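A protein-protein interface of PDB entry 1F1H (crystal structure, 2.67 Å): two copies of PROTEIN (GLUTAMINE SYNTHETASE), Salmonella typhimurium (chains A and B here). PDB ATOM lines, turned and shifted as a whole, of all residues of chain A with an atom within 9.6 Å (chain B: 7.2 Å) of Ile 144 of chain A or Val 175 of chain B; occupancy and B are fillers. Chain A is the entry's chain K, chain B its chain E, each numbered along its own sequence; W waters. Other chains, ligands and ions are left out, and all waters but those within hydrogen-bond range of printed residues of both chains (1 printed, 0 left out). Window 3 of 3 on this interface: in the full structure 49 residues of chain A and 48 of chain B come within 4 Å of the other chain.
The backbone carbonyl oxygen (O) of Pro 457 of chain A sits at hydrogen-bond distance from the side-chain hydroxyl (OG) of Ser 147 of chain A, at 3.5 Å.
OG of Ser 143 of chain A is in hydrogen-bond range of OG of Ser 145 of chain A, at 3.2 Å.
Water W1 lies within hydrogen-bond range of the backbone carbonyl oxygen of Ile 144 of chain A (2.7 Å), the backbone NH of Phe 261 of chain B (2.9 Å) and the backbone carbonyl oxygen of Ser 143 of chain A (3.2 Å).
Ile 144 of chain A touches four residues of chain B.
Of the printed residues of chain B, Pro 457 of chain A touches Pro 259 (3.7 Å) and Phe 261 (3.6 Å).
Of the printed residues of chain B, Phe 462 of chain A touches Pro 259.
Printed residues of chain A within 4 Å of Ile 151 of chain B: Ser 145.
Gly 174 of chain B touches none of the printed residues of chain A.
Of the printed residues of chain A, Val 175 of chain B touches Ile 144.
Of the printed residues of chain A, Met 260 of chain B touches Ile 144.
The nearest printed residue of chain B that does not touch Ser 145 of chain A is Met 260 of chain B (4.9 Å).
No position is printed for both chains.
Of the 9 pairs that touch across the chains among the printed residues, none has its exchanged pair printed and touching as well.
N of Ile 151 of chain B lies within hydrogen-bond range of O of Ser 145 of chain A, 2.8 Å away.
Of the 20 printed residues of chain B, 6 touch a printed residue of chain A.
Printed residues of chain B that touch a printed residue of chain A: Ile 151, Trp 158, Val 175, Pro 259, Met 260 and Phe 261.
Hydrophobic or aromatic side chains of chain B within 4 Å of the printed part of chain A: Ile 151, Trp 158, Val 175, Met 260 and Phe 261.
Among the printed residues, 9 pairs touch across the chains.
Among the printed residues, no Asp or Glu carboxylate lies within 4 Å of a Lys or Arg side-chain nitrogen of the other chain.
Among the printed residues, pairs that only touch across the chains: Ile 144 of chain A with Met 260 of chain B, Phe 462 of chain A with Pro 259 of chain B, Ile 144 of chain A with Phe 261 of chain B, Pro 457 of chain A with Phe 261 of chain B, Ile 144 of chain A with Trp 158 of chain B, Ser 145 of chain A with Trp 158 of chain B, Pro 457 of chain A with Pro 259 of chain B and Ile 144 of chain A with Val 175 of chain B.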
ATOM      1  N   GLY A 141       3.068 -17.395 -28.396  1.00  0.00           N
ATOM      2  CA  GLY A 141       3.234 -18.794 -28.063  1.00  0.00           C
ATOM      3  C   GLY A 141       2.882 -19.066 -26.622  1.00  0.00           C
ATOM      4  O   GLY A 141       2.786 -18.138 -25.812  1.00  0.00           O
ATOM      5  N   ALA A 142       2.684 -20.343 -26.309  1.00  0.00           N
ATOM      6  CA  ALA A 142       2.352 -20.774 -24.956  1.00  0.00           C
ATOM      7  C   ALA A 142       2.819 -22.202 -24.793  1.00  0.00           C
ATOM      8  O   ALA A 142       2.547 -23.060 -25.642  1.00  0.00           O
ATOM      9  CB  ALA A 142       0.866 -20.687 -24.714  1.00  0.00           C
ATOM     10  N   SER A 143       3.583 -22.424 -23.732  1.00  0.00           N
ATOM     11  CA  SER A 143       4.123 -23.733 -23.401  1.00  0.00           C
ATOM     12  C   SER A 143       4.096 -23.826 -21.882  1.00  0.00           C
ATOM     13  O   SER A 143       3.728 -22.863 -21.200  1.00  0.00           O
ATOM     14  CB  SER A 143       5.547 -23.889 -23.943  1.00  0.00           C
ATOM     15  OG  SER A 143       6.519 -23.305 -23.093  1.00  0.00           O
ATOM     16  N   ILE A 144       4.495 -24.972 -21.347  1.00  0.00           N
ATOM     17  CA  ILE A 144       4.474 -25.165 -19.902  1.00  0.00           C
ATOM     18  C   ILE A 144       5.269 -24.103 -19.128  1.00  0.00           C
ATOM     19  O   ILE A 144       4.841 -23.664 -18.071  1.00  0.00           O
ATOM     20  CB  ILE A 144       4.935 -26.596 -19.524  1.00  0.00           C
ATOM     21  CG1 ILE A 144       4.748 -26.837 -18.027  1.00  0.00           C
ATOM     22  CG2 ILE A 144       6.380 -26.830 -19.941  1.00  0.00           C
ATOM     23  CD1 ILE A 144       5.200 -28.210 -17.560  1.00  0.00           C
ATOM     24  N   SER A 145       6.385 -23.649 -19.689  1.00  0.00           N
ATOM     25  CA  SER A 145       7.238 -22.645 -19.043  1.00  0.00           C
ATOM     26  C   SER A 145       6.837 -21.171 -19.213  1.00  0.00           C
ATOM     27  O   SER A 145       7.488 -20.288 -18.645  1.00  0.00           O
ATOM     28  CB  SER A 145       8.703 -22.829 -19.472  1.00  0.00           C
ATOM     29  OG  SER A 145       8.838 -22.940 -20.878  1.00  0.00           O
ATOM     30  N   GLY A 146       5.789 -20.900 -19.992  1.00  0.00           N
ATOM     31  CA  GLY A 146       5.361 -19.519 -20.189  1.00  0.00           C
ATOM     32  C   GLY A 146       4.473 -19.255 -21.395  1.00  0.00           C
ATOM     33  O   GLY A 146       3.998 -20.177 -22.070  1.00  0.00           O
ATOM     34  N   SER A 147       4.260 -17.972 -21.668  1.00  0.00           N
ATOM     35  CA  SER A 147       3.431 -17.515 -22.780  1.00  0.00           C
ATOM     36  C   SER A 147       3.924 -16.147 -23.169  1.00  0.00           C
ATOM     37  O   SER A 147       4.610 -15.487 -22.389  1.00  0.00           O
ATOM     38  CB  SER A 147       1.941 -17.379 -22.371  1.00  0.00           C
ATOM     39  OG  SER A 147       1.721 -17.405 -20.954  1.00  0.00           O
ATOM     40  N   ARG A 452      -9.137 -22.826 -22.814  1.00  0.00           N
ATOM     41  CA  ARG A 452      -7.720 -22.560 -22.973  1.00  0.00           C
ATOM     42  C   ARG A 452      -7.336 -21.244 -22.330  1.00  0.00           C
ATOM     43  O   ARG A 452      -6.341 -21.150 -21.616  1.00  0.00           O
ATOM     44  CB  ARG A 452      -7.329 -22.579 -24.448  1.00  0.00           C
ATOM     45  CG  ARG A 452      -7.360 -23.970 -25.061  1.00  0.00           C
ATOM     46  CD  ARG A 452      -6.278 -24.127 -26.109  1.00  0.00           C
ATOM     47  NE  ARG A 452      -4.982 -23.748 -25.556  1.00  0.00           N
ATOM     48  CZ  ARG A 452      -3.949 -23.329 -26.277  1.00  0.00           C
ATOM     49  NH1 ARG A 452      -2.816 -23.000 -25.659  1.00  0.00           N
ATOM     50  NH2 ARG A 452      -4.042 -23.256 -27.607  1.00  0.00           N
ATOM     51  N   THR A 456      -5.037 -21.241 -18.799  1.00  0.00           N
ATOM     52  CA  THR A 456      -3.631 -20.852 -18.991  1.00  0.00           C
ATOM     53  C   THR A 456      -3.203 -19.595 -18.222  1.00  0.00           C
ATOM     54  O   THR A 456      -3.731 -18.516 -18.464  1.00  0.00           O
ATOM     55  CB  THR A 456      -3.346 -20.601 -20.494  1.00  0.00           C
ATOM     56  OG1 THR A 456      -3.654 -21.777 -21.258  1.00  0.00           O
ATOM     57  CG2 THR A 456      -1.901 -20.218 -20.710  1.00  0.00           C
ATOM     58  N   PRO A 457      -2.182 -19.699 -17.350  1.00  0.00           N
ATOM     59  CA  PRO A 457      -1.740 -18.519 -16.596  1.00  0.00           C
ATOM     60  C   PRO A 457      -1.438 -17.345 -17.530  1.00  0.00           C
ATOM     61  O   PRO A 457      -0.806 -17.514 -18.577  1.00  0.00           O
ATOM     62  CB  PRO A 457      -0.476 -19.014 -15.896  1.00  0.00           C
ATOM     63  CG  PRO A 457      -0.744 -20.452 -15.691  1.00  0.00           C
ATOM     64  CD  PRO A 457      -1.356 -20.867 -17.010  1.00  0.00           C
ATOM     65  N   PHE A 462       1.359 -12.607 -13.062  1.00  0.00           N
ATOM     66  CA  PHE A 462       2.667 -12.632 -12.444  1.00  0.00           C
ATOM     67  C   PHE A 462       3.013 -11.264 -11.903  1.00  0.00           C
ATOM     68  O   PHE A 462       3.599 -11.134 -10.822  1.00  0.00           O
ATOM     69  CB  PHE A 462       3.725 -13.114 -13.455  1.00  0.00           C
ATOM     70  CG  PHE A 462       3.510 -14.570 -13.770  1.00  0.00           C
ATOM     71  CD1 PHE A 462       4.251 -15.532 -13.081  1.00  0.00           C
ATOM     72  CD2 PHE A 462       2.574 -14.990 -14.707  1.00  0.00           C
ATOM     73  CE1 PHE A 462       4.040 -16.887 -13.314  1.00  0.00           C
ATOM     74  CE2 PHE A 462       2.368 -16.356 -14.943  1.00  0.00           C
ATOM     75  CZ  PHE A 462       3.087 -17.295 -14.250  1.00  0.00           C
ATOM     76  N   ILE B 151       9.333 -18.670 -17.298  1.00  0.00           N
ATOM     77  CA  ILE B 151       9.779 -19.331 -16.072  1.00  0.00           C
ATOM     78  C   ILE B 151      10.945 -20.227 -16.407  1.00  0.00           C
ATOM     79  O   ILE B 151      10.983 -20.852 -17.466  1.00  0.00           O
ATOM     80  CB  ILE B 151       8.675 -20.253 -15.500  1.00  0.00           C
ATOM     81  CG1 ILE B 151       7.506 -19.433 -15.006  1.00  0.00           C
ATOM     82  CG2 ILE B 151       9.191 -21.083 -14.355  1.00  0.00           C
ATOM     83  CD1 ILE B 151       6.314 -20.254 -14.785  1.00  0.00           C
ATOM     84  N   ALA B 157      11.554 -29.691 -16.678  1.00  0.00           N
ATOM     85  CA  ALA B 157      11.687 -30.782 -17.633  1.00  0.00           C
ATOM     86  C   ALA B 157      12.086 -30.317 -19.028  1.00  0.00           C
ATOM     87  O   ALA B 157      12.709 -31.065 -19.790  1.00  0.00           O
ATOM     88  CB  ALA B 157      10.413 -31.557 -17.687  1.00  0.00           C
ATOM     89  N   TRP B 158      11.732 -29.074 -19.345  1.00  0.00           N
ATOM     90  CA  TRP B 158      12.041 -28.481 -20.641  1.00  0.00           C
ATOM     91  C   TRP B 158      13.525 -28.253 -20.853  1.00  0.00           C
ATOM     92  O   TRP B 158      13.957 -28.017 -21.986  1.00  0.00           O
ATOM     93  CB  TRP B 158      11.297 -27.154 -20.829  1.00  0.00           C
ATOM     94  CG  TRP B 158      11.527 -26.148 -19.734  1.00  0.00           C
ATOM     95  CD1 TRP B 158      12.553 -25.246 -19.636  1.00  0.00           C
ATOM     96  CD2 TRP B 158      10.696 -25.934 -18.585  1.00  0.00           C
ATOM     97  NE1 TRP B 158      12.412 -24.481 -18.497  1.00  0.00           N
ATOM     98  CE2 TRP B 158      11.279 -24.882 -17.833  1.00  0.00           C
ATOM     99  CE3 TRP B 158       9.512 -26.528 -18.117  1.00  0.00           C
ATOM    100  CZ2 TRP B 158      10.715 -24.410 -16.635  1.00  0.00           C
ATOM    101  CZ3 TRP B 158       8.950 -26.056 -16.924  1.00  0.00           C
ATOM    102  CH2 TRP B 158       9.556 -25.006 -16.201  1.00  0.00           C
ATOM    103  N   ARG B 172      16.393 -34.690 -13.862  1.00  0.00           N
ATOM    104  CA  ARG B 172      15.331 -33.813 -13.435  1.00  0.00           C
ATOM    105  C   ARG B 172      13.968 -34.447 -13.484  1.00  0.00           C
ATOM    106  O   ARG B 172      13.717 -35.384 -14.245  1.00  0.00           O
ATOM    107  CB  ARG B 172      15.356 -32.477 -14.196  1.00  0.00           C
ATOM    108  CG  ARG B 172      15.665 -32.544 -15.666  1.00  0.00           C
ATOM    109  CD  ARG B 172      15.715 -31.144 -16.284  1.00  0.00           C
ATOM    110  NE  ARG B 172      16.925 -30.328 -16.052  1.00  0.00           N
ATOM    111  CZ  ARG B 172      18.097 -30.503 -16.671  1.00  0.00           C
ATOM    112  NH1 ARG B 172      19.111 -29.676 -16.431  1.00  0.00           N
ATOM    113  NH2 ARG B 172      18.302 -31.571 -17.436  1.00  0.00           N
ATOM    114  N   PRO B 173      13.075 -33.963 -12.614  1.00  0.00           N
ATOM    115  CA  PRO B 173      11.707 -34.456 -12.519  1.00  0.00           C
ATOM    116  C   PRO B 173      10.892 -34.105 -13.759  1.00  0.00           C
ATOM    117  O   PRO B 173      10.893 -32.947 -14.206  1.00  0.00           O
ATOM    118  CB  PRO B 173      11.183 -33.726 -11.275  1.00  0.00           C
ATOM    119  CG  PRO B 173      11.909 -32.422 -11.307  1.00  0.00           C
ATOM    120  CD  PRO B 173      13.311 -32.867 -11.651  1.00  0.00           C
ATOM    121  N   GLY B 174      10.245 -35.111 -14.342  1.00  0.00           N
ATOM    122  CA  GLY B 174       9.396 -34.867 -15.499  1.00  0.00           C
ATOM    123  C   GLY B 174       8.100 -34.173 -15.059  1.00  0.00           C
ATOM    124  O   GLY B 174       7.886 -33.924 -13.866  1.00  0.00           O
ATOM    125  N   VAL B 175       7.232 -33.846 -16.012  1.00  0.00           N
ATOM    126  CA  VAL B 175       5.964 -33.182 -15.699  1.00  0.00           C
ATOM    127  C   VAL B 175       5.147 -34.072 -14.756  1.00  0.00           C
ATOM    128  O   VAL B 175       4.967 -35.264 -15.031  1.00  0.00           O
ATOM    129  CB  VAL B 175       5.170 -32.890 -17.003  1.00  0.00           C
ATOM    130  CG1 VAL B 175       3.833 -32.224 -16.695  1.00  0.00           C
ATOM    131  CG2 VAL B 175       5.988 -31.992 -17.908  1.00  0.00           C
ATOM    132  N   LYS B 176       4.689 -33.495 -13.642  1.00  0.00           N
ATOM    133  CA  LYS B 176       3.908 -34.219 -12.624  1.00  0.00           C
ATOM    134  C   LYS B 176       4.709 -35.377 -11.998  1.00  0.00           C
ATOM    135  O   LYS B 176       4.134 -36.238 -11.332  1.00  0.00           O
ATOM    136  CB  LYS B 176       2.594 -34.789 -13.210  1.00  0.00           C
ATOM    137  CG  LYS B 176       1.413 -33.825 -13.373  1.00  0.00           C
ATOM    138  CD  LYS B 176       0.153 -34.606 -13.784  1.00  0.00           C
ATOM    139  CE  LYS B 176      -1.113 -33.744 -13.852  1.00  0.00           C
ATOM    140  NZ  LYS B 176      -1.202 -32.904 -15.084  1.00  0.00           N
ATOM    141  N   GLY B 177       6.029 -35.379 -12.167  1.00  0.00           N
ATOM    142  CA  GLY B 177       6.823 -36.478 -11.640  1.00  0.00           C
ATOM    143  C   GLY B 177       7.825 -36.152 -10.557  1.00  0.00           C
ATOM    144  O   GLY B 177       8.774 -36.917 -10.310  1.00  0.00           O
ATOM    145  N   GLY B 178       7.740 -34.966  -9.943  1.00  0.00           N
ATOM    146  CA  GLY B 178       8.772 -34.563  -8.999  1.00  0.00           C
ATOM    147  C   GLY B 178       8.485 -35.099  -7.647  1.00  0.00           C
ATOM    148  O   GLY B 178       9.000 -34.656  -6.619  1.00  0.00           O
ATOM    149  N   VAL B 213       4.625 -32.470  -6.382  1.00  0.00           N
ATOM    150  CA  VAL B 213       4.355 -33.068  -7.688  1.00  0.00           C
ATOM    151  C   VAL B 213       4.903 -32.407  -8.959  1.00  0.00           C
ATOM    152  O   VAL B 213       5.429 -33.073  -9.855  1.00  0.00           O
ATOM    153  CB  VAL B 213       2.845 -33.267  -7.864  1.00  0.00           C
ATOM    154  CG1 VAL B 213       2.530 -33.861  -9.216  1.00  0.00           C
ATOM    155  CG2 VAL B 213       2.331 -34.144  -6.790  1.00  0.00           C
ATOM    156  N   ALA B 214       4.774 -31.099  -9.058  1.00  0.00           N
ATOM    157  CA  ALA B 214       5.216 -30.433 -10.262  1.00  0.00           C
ATOM    158  C   ALA B 214       6.721 -30.425 -10.513  1.00  0.00           C
ATOM    159  O   ALA B 214       7.532 -30.560  -9.591  1.00  0.00           O
ATOM    160  CB  ALA B 214       4.661 -29.013 -10.298  1.00  0.00           C
ATOM    161  N   THR B 215       7.075 -30.328 -11.792  1.00  0.00           N
ATOM    162  CA  THR B 215       8.463 -30.228 -12.214  1.00  0.00           C
ATOM    163  C   THR B 215       8.847 -28.768 -11.900  1.00  0.00           C
ATOM    164  O   THR B 215       8.051 -28.010 -11.336  1.00  0.00           O
ATOM    165  CB  THR B 215       8.603 -30.490 -13.748  1.00  0.00           C
ATOM    166  OG1 THR B 215       9.981 -30.403 -14.140  1.00  0.00           O
ATOM    167  CG2 THR B 215       7.798 -29.480 -14.565  1.00  0.00           C
ATOM    168  N   ALA B 216      10.068 -28.379 -12.221  1.00  0.00           N
ATOM    169  CA  ALA B 216      10.505 -27.008 -12.015  1.00  0.00           C
ATOM    170  C   ALA B 216      10.396 -26.504 -10.583  1.00  0.00           C
ATOM    171  O   ALA B 216      10.084 -25.345 -10.375  1.00  0.00           O
ATOM    172  CB  ALA B 216       9.718 -26.105 -12.955  1.00  0.00           C
ATOM    173  N   PRO B 259       1.486 -21.216 -11.436  1.00  0.00           N
ATOM    174  CA  PRO B 259       2.452 -20.587 -12.338  1.00  0.00           C
ATOM    175  C   PRO B 259       2.528 -21.220 -13.731  1.00  0.00           C
ATOM    176  O   PRO B 259       2.823 -20.537 -14.718  1.00  0.00           O
ATOM    177  CB  PRO B 259       3.774 -20.734 -11.571  1.00  0.00           C
ATOM    178  CG  PRO B 259       3.570 -21.966 -10.752  1.00  0.00           C
ATOM    179  CD  PRO B 259       2.154 -21.812 -10.263  1.00  0.00           C
ATOM    180  N   MET B 260       2.221 -22.513 -13.812  1.00  0.00           N
ATOM    181  CA  MET B 260       2.293 -23.250 -15.076  1.00  0.00           C
ATOM    182  C   MET B 260       1.057 -24.042 -15.466  1.00  0.00           C
ATOM    183  O   MET B 260       0.470 -24.746 -14.649  1.00  0.00           O
ATOM    184  CB  MET B 260       3.454 -24.246 -15.048  1.00  0.00           C
ATOM    185  CG  MET B 260       4.828 -23.640 -14.909  1.00  0.00           C
ATOM    186  SD  MET B 260       6.084 -24.899 -14.637  1.00  0.00           S
ATOM    187  CE  MET B 260       5.750 -25.301 -12.927  1.00  0.00           C
ATOM    188  N   PHE B 261       0.697 -23.960 -16.739  1.00  0.00           N
ATOM    189  CA  PHE B 261      -0.414 -24.729 -17.248  1.00  0.00           C
ATOM    190  C   PHE B 261       0.143 -26.121 -17.562  1.00  0.00           C
ATOM    191  O   PHE B 261       1.194 -26.253 -18.199  1.00  0.00           O
ATOM    192  CB  PHE B 261      -0.971 -24.119 -18.539  1.00  0.00           C
ATOM    193  CG  PHE B 261      -1.940 -25.024 -19.252  1.00  0.00           C
ATOM    194  CD1 PHE B 261      -3.235 -25.194 -18.774  1.00  0.00           C
ATOM    195  CD2 PHE B 261      -1.531 -25.782 -20.345  1.00  0.00           C
ATOM    196  CE1 PHE B 261      -4.110 -26.111 -19.365  1.00  0.00           C
ATOM    197  CE2 PHE B 261      -2.401 -26.703 -20.941  1.00  0.00           C
ATOM    198  CZ  PHE B 261      -3.690 -26.865 -20.445  1.00  0.00           C
ATOM    199  N   GLY B 262      -0.548 -27.161 -17.113  1.00  0.00           N
ATOM    200  CA  GLY B 262      -0.086 -28.498 -17.427  1.00  0.00           C
ATOM    201  C   GLY B 262       0.600 -29.232 -16.309  1.00  0.00           C
ATOM    202  O   GLY B 262       1.031 -30.366 -16.494  1.00  0.00           O
ATOM    203  N   ASP B 263       0.808 -28.556 -15.191  1.00  0.00           N
ATOM    204  CA  ASP B 263       1.405 -29.209 -14.048  1.00  0.00           C
ATOM    205  C   ASP B 263       0.689 -28.696 -12.821  1.00  0.00           C
ATOM    206  O   ASP B 263      -0.118 -27.773 -12.900  1.00  0.00           O
ATOM    207  CB  ASP B 263       2.920 -28.986 -13.952  1.00  0.00           C
ATOM    208  CG  ASP B 263       3.657 -30.198 -13.349  1.00  0.00           C
ATOM    209  OD1 ASP B 263       4.848 -30.406 -13.654  1.00  0.00           O
ATOM    210  OD2 ASP B 263       3.049 -30.966 -12.578  1.00  0.00           O
ATOM    211  N   ASN B 264       0.927 -29.378 -11.711  1.00  0.00           N
ATOM    212  CA  ASN B 264       0.341 -29.071 -10.418  1.00  0.00           C
ATOM    213  C   ASN B 264       0.377 -27.602 -10.022  1.00  0.00           C
ATOM    214  O   ASN B 264       1.348 -26.890 -10.309  1.00  0.00           O
ATOM    215  CB  ASN B 264       1.122 -29.834  -9.356  1.00  0.00           C
ATOM    216  CG  ASN B 264       0.264 -30.750  -8.538  1.00  0.00           C
ATOM    217  OD1 ASN B 264       0.447 -30.847  -7.317  1.00  0.00           O
ATOM    218  ND2 ASN B 264      -0.646 -31.471  -9.202  1.00  0.00           N
HETATM  219  O   HOH W   1       2.499 -22.358 -18.265  1.00  0.00           O
